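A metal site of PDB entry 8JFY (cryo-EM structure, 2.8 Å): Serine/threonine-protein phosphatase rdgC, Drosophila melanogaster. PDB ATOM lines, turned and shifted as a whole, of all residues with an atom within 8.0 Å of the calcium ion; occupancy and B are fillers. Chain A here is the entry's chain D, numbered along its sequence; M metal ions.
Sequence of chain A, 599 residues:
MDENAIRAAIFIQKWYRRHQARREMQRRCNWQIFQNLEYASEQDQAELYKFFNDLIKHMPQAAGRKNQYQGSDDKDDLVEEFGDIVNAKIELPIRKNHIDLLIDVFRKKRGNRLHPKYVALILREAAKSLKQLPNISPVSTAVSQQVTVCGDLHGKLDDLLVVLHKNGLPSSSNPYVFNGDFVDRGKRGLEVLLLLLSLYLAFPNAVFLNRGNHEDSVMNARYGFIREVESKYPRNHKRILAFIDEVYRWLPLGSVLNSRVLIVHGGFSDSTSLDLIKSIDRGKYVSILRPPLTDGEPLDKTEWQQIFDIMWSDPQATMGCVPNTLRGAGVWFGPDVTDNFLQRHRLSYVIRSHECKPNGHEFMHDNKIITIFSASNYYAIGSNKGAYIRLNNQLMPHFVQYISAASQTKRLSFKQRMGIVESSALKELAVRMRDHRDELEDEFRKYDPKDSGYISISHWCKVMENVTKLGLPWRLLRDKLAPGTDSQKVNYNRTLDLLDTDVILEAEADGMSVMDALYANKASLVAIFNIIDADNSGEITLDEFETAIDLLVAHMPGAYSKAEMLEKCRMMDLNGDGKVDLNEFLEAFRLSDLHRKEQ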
ATOM      1  N   PHE A 529      26.032 -26.354 -15.666  1.00  0.00           N
ATOM      2  CA  PHE A 529      26.027 -25.195 -16.559  1.00  0.00           C
ATOM      3  C   PHE A 529      25.389 -23.985 -15.887  1.00  0.00           C
ATOM      4  O   PHE A 529      25.885 -22.860 -16.033  1.00  0.00           O
ATOM      5  CB  PHE A 529      25.295 -25.541 -17.854  1.00  0.00           C
ATOM      6  CG  PHE A 529      25.333 -24.447 -18.882  1.00  0.00           C
ATOM      7  CD1 PHE A 529      26.439 -24.295 -19.715  1.00  0.00           C
ATOM      8  CD2 PHE A 529      24.275 -23.574 -19.026  1.00  0.00           C
ATOM      9  CE1 PHE A 529      26.476 -23.288 -20.657  1.00  0.00           C
ATOM     10  CE2 PHE A 529      24.307 -22.561 -19.975  1.00  0.00           C
ATOM     11  CZ  PHE A 529      25.413 -22.426 -20.794  1.00  0.00           C
ATOM     12  N   ILE A 532      27.952 -22.582 -13.499  1.00  0.00           N
ATOM     13  CA  ILE A 532      29.013 -21.821 -14.147  1.00  0.00           C
ATOM     14  C   ILE A 532      28.479 -20.608 -14.911  1.00  0.00           C
ATOM     15  O   ILE A 532      29.269 -19.746 -15.310  1.00  0.00           O
ATOM     16  CB  ILE A 532      29.841 -22.709 -15.083  1.00  0.00           C
ATOM     17  CG1 ILE A 532      29.026 -23.110 -16.307  1.00  0.00           C
ATOM     18  CG2 ILE A 532      30.338 -23.939 -14.340  1.00  0.00           C
ATOM     19  CD1 ILE A 532      29.838 -23.796 -17.394  1.00  0.00           C
ATOM     20  N   ASP A 533      27.169 -20.526 -15.125  1.00  0.00           N
ATOM     21  CA  ASP A 533      26.581 -19.375 -15.796  1.00  0.00           C
ATOM     22  C   ASP A 533      26.276 -18.279 -14.786  1.00  0.00           C
ATOM     23  O   ASP A 533      25.130 -18.127 -14.343  1.00  0.00           O
ATOM     24  CB  ASP A 533      25.318 -19.784 -16.551  1.00  0.00           C
ATOM     25  CG  ASP A 533      24.889 -18.766 -17.590  1.00  0.00           C
ATOM     26  OD1 ASP A 533      25.776 -18.122 -18.193  1.00  0.00           O
ATOM     27  OD2 ASP A 533      23.671 -18.606 -17.805  1.00  0.00           O
ATOM     28  N   ALA A 534      27.301 -17.503 -14.415  1.00  0.00           N
ATOM     29  CA  ALA A 534      27.161 -16.526 -13.340  1.00  0.00           C
ATOM     30  C   ALA A 534      26.182 -15.415 -13.698  1.00  0.00           C
ATOM     31  O   ALA A 534      25.345 -15.036 -12.863  1.00  0.00           O
ATOM     32  CB  ALA A 534      28.525 -15.932 -12.983  1.00  0.00           C
ATOM     33  N   ASP A 535      26.267 -14.878 -14.912  1.00  0.00           N
ATOM     34  CA  ASP A 535      25.422 -13.752 -15.293  1.00  0.00           C
ATOM     35  C   ASP A 535      24.046 -14.169 -15.792  1.00  0.00           C
ATOM     36  O   ASP A 535      23.228 -13.297 -16.100  1.00  0.00           O
ATOM     37  CB  ASP A 535      26.128 -12.900 -16.371  1.00  0.00           C
ATOM     38  CG  ASP A 535      26.370 -13.656 -17.674  1.00  0.00           C
ATOM     39  OD1 ASP A 535      25.836 -14.765 -17.860  1.00  0.00           O
ATOM     40  OD2 ASP A 535      27.122 -13.121 -18.516  1.00  0.00           O
ATOM     41  N   ASN A 536      23.774 -15.468 -15.886  1.00  0.00           N
ATOM     42  CA  ASN A 536      22.513 -16.037 -16.350  1.00  0.00           C
ATOM     43  C   ASN A 536      22.185 -15.660 -17.787  1.00  0.00           C
ATOM     44  O   ASN A 536      21.048 -15.839 -18.226  1.00  0.00           O
ATOM     45  CB  ASN A 536      21.354 -15.644 -15.422  1.00  0.00           C
ATOM     46  CG  ASN A 536      21.387 -16.390 -14.093  1.00  0.00           C
ATOM     47  OD1 ASN A 536      20.453 -16.315 -13.298  1.00  0.00           O
ATOM     48  ND2 ASN A 536      22.469 -17.136 -13.859  1.00  0.00           N
ATOM     49  N   SER A 537      23.158 -15.129 -18.531  1.00  0.00           N
ATOM     50  CA  SER A 537      22.951 -14.824 -19.940  1.00  0.00           C
ATOM     51  C   SER A 537      22.933 -16.101 -20.764  1.00  0.00           C
ATOM     52  O   SER A 537      23.474 -17.132 -20.333  1.00  0.00           O
ATOM     53  CB  SER A 537      24.033 -13.878 -20.448  1.00  0.00           C
ATOM     54  OG  SER A 537      23.835 -13.550 -21.814  1.00  0.00           O
ATOM     55  N   GLY A 538      22.305 -16.044 -21.928  1.00  0.00           N
ATOM     56  CA  GLY A 538      22.212 -17.210 -22.788  1.00  0.00           C
ATOM     57  C   GLY A 538      23.560 -17.645 -23.335  1.00  0.00           C
ATOM     58  O   GLY A 538      24.501 -16.860 -23.487  1.00  0.00           O
ATOM     59  N   GLU A 539      23.634 -18.943 -23.650  1.00  0.00           N
ATOM     60  CA  GLU A 539      24.796 -19.605 -24.237  1.00  0.00           C
ATOM     61  C   GLU A 539      26.116 -19.122 -23.624  1.00  0.00           C
ATOM     62  O   GLU A 539      27.080 -18.828 -24.331  1.00  0.00           O
ATOM     63  CB  GLU A 539      24.800 -19.473 -25.765  1.00  0.00           C
ATOM     64  CG  GLU A 539      24.856 -18.058 -26.329  1.00  0.00           C
ATOM     65  CD  GLU A 539      25.001 -18.028 -27.836  1.00  0.00           C
ATOM     66  OE1 GLU A 539      24.539 -18.981 -28.498  1.00  0.00           O
ATOM     67  OE2 GLU A 539      25.582 -17.053 -28.363  1.00  0.00           O
ATOM     68  N   ILE A 540      26.144 -19.072 -22.288  1.00  0.00           N
ATOM     69  CA  ILE A 540      27.314 -18.792 -21.461  1.00  0.00           C
ATOM     70  C   ILE A 540      28.064 -17.549 -21.949  1.00  0.00           C
ATOM     71  O   ILE A 540      27.508 -16.734 -22.703  1.00  0.00           O
ATOM     72  CB  ILE A 540      28.228 -20.043 -21.377  1.00  0.00           C
ATOM     73  CG1 ILE A 540      29.009 -20.074 -20.065  1.00  0.00           C
ATOM     74  CG2 ILE A 540      29.171 -20.174 -22.590  1.00  0.00           C
ATOM     75  CD1 ILE A 540      28.194 -20.547 -18.884  1.00  0.00           C
ATOM     76  N   THR A 541      29.308 -17.367 -21.496  1.00  0.00           N
ATOM     77  CA  THR A 541      30.137 -16.241 -21.898  1.00  0.00           C
ATOM     78  C   THR A 541      31.594 -16.649 -21.753  1.00  0.00           C
ATOM     79  O   THR A 541      31.943 -17.407 -20.850  1.00  0.00           O
ATOM     80  CB  THR A 541      29.852 -14.997 -21.044  1.00  0.00           C
ATOM     81  OG1 THR A 541      28.432 -14.800 -20.933  1.00  0.00           O
ATOM     82  CG2 THR A 541      30.471 -13.757 -21.658  1.00  0.00           C
ATOM     83  N   LEU A 542      32.439 -16.146 -22.659  1.00  0.00           N
ATOM     84  CA  LEU A 542      33.875 -16.416 -22.571  1.00  0.00           C
ATOM     85  C   LEU A 542      34.462 -15.818 -21.299  1.00  0.00           C
ATOM     86  O   LEU A 542      35.366 -16.401 -20.690  1.00  0.00           O
ATOM     87  CB  LEU A 542      34.585 -15.859 -23.809  1.00  0.00           C
ATOM     88  CG  LEU A 542      36.075 -16.179 -23.990  1.00  0.00           C
ATOM     89  CD1 LEU A 542      36.391 -17.609 -23.534  1.00  0.00           C
ATOM     90  CD2 LEU A 542      36.491 -15.976 -25.436  1.00  0.00           C
ATOM     91  N   ASP A 543      33.948 -14.653 -20.875  1.00  0.00           N
ATOM     92  CA  ASP A 543      34.376 -14.070 -19.608  1.00  0.00           C
ATOM     93  C   ASP A 543      34.045 -14.993 -18.447  1.00  0.00           C
ATOM     94  O   ASP A 543      34.853 -15.161 -17.530  1.00  0.00           O
ATOM     95  CB  ASP A 543      33.723 -12.701 -19.419  1.00  0.00           C
ATOM     96  CG  ASP A 543      33.890 -11.803 -20.622  1.00  0.00           C
ATOM     97  OD1 ASP A 543      34.245 -12.311 -21.701  1.00  0.00           O
ATOM     98  OD2 ASP A 543      33.667 -10.572 -20.489  1.00  0.00           O
ATOM     99  N   GLU A 544      32.862 -15.618 -18.479  1.00  0.00           N
ATOM    100  CA  GLU A 544      32.524 -16.607 -17.465  1.00  0.00           C
ATOM    101  C   GLU A 544      33.476 -17.791 -17.516  1.00  0.00           C
ATOM    102  O   GLU A 544      33.876 -18.317 -16.467  1.00  0.00           O
ATOM    103  CB  GLU A 544      31.083 -17.082 -17.638  1.00  0.00           C
ATOM    104  CG  GLU A 544      30.054 -16.169 -17.005  1.00  0.00           C
ATOM    105  CD  GLU A 544      28.635 -16.520 -17.413  1.00  0.00           C
ATOM    106  OE1 GLU A 544      28.454 -17.056 -18.525  1.00  0.00           O
ATOM    107  OE2 GLU A 544      27.709 -16.278 -16.612  1.00  0.00           O
ATOM    108  N   PHE A 545      33.865 -18.226 -18.723  1.00  0.00           N
ATOM    109  CA  PHE A 545      34.785 -19.346 -18.846  1.00  0.00           C
ATOM    110  C   PHE A 545      36.127 -19.020 -18.204  1.00  0.00           C
ATOM    111  O   PHE A 545      36.675 -19.823 -17.422  1.00  0.00           O
ATOM    112  CB  PHE A 545      34.974 -19.721 -20.314  1.00  0.00           C
ATOM    113  CG  PHE A 545      34.000 -20.753 -20.796  1.00  0.00           C
ATOM    114  CD1 PHE A 545      33.779 -21.920 -20.079  1.00  0.00           C
ATOM    115  CD2 PHE A 545      33.309 -20.567 -21.990  1.00  0.00           C
ATOM    116  CE1 PHE A 545      32.893 -22.867 -20.527  1.00  0.00           C
ATOM    117  CE2 PHE A 545      32.415 -21.520 -22.438  1.00  0.00           C
ATOM    118  CZ  PHE A 545      32.207 -22.670 -21.713  1.00  0.00           C
ATOM    119  N   LYS A 579      30.534 -19.023 -28.298  1.00  0.00           N
ATOM    120  CA  LYS A 579      29.730 -19.208 -27.098  1.00  0.00           C
ATOM    121  C   LYS A 579      29.263 -20.646 -27.027  1.00  0.00           C
ATOM    122  O   LYS A 579      29.185 -21.351 -28.039  1.00  0.00           O
ATOM    123  CB  LYS A 579      28.532 -18.232 -27.079  1.00  0.00           C
ATOM    124  CG  LYS A 579      28.849 -16.883 -26.462  1.00  0.00           C
ATOM    125  CD  LYS A 579      29.447 -15.924 -27.477  1.00  0.00           C
ATOM    126  CE  LYS A 579      28.408 -15.452 -28.480  1.00  0.00           C
ATOM    127  NZ  LYS A 579      29.019 -14.655 -29.578  1.00  0.00           N
ATOM    128  N   VAL A 580      28.939 -21.096 -25.820  1.00  0.00           N
ATOM    129  CA  VAL A 580      28.540 -22.488 -25.595  1.00  0.00           C
ATOM    130  C   VAL A 580      27.153 -22.531 -24.980  1.00  0.00           C
ATOM    131  O   VAL A 580      26.955 -22.130 -23.823  1.00  0.00           O
ATOM    132  CB  VAL A 580      29.559 -23.221 -24.709  1.00  0.00           C
ATOM    133  CG1 VAL A 580      29.178 -24.678 -24.561  1.00  0.00           C
ATOM    134  CG2 VAL A 580      30.965 -23.080 -25.282  1.00  0.00           C
HETATM  135 CA    CA M   1      26.537 -16.213 -19.817  1.00  0.00          CA
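OD1 of Asp 535 sits close to N of Ser 537. The backbone carbonyl oxygen of Asp 533 lies within hydrogen-bond range of the side-chain amide nitrogen of Asn 536 (2.9 Å). OE2 of Glu 544 sits at hydrogen-bond distance from N of Ala 534.
Ser 537 touches the calcium ion. Of the 17 residues printed, 6 come within 4 Å of the calcium ion. The nearest printed residue that does not touch the calcium ion is Gly 538 (4.2 Å).
The calcium ion is bound by the side-chain carboxylate (OE1) of Glu 544 (2.5 Å), the side-chain carboxylate (OD1) of Asp 535 (2.5 Å), the side-chain hydroxyl (OG1) of Thr 541 (2.6 Å) and the side-chain carboxylate (OD1) of Asp 533 (2.6 Å). The calcium ion has four donor atoms within binding distance. Slightly farther from the calcium ion lies the backbone carbonyl oxygen (O) of Ile 540 (3.1 Å).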
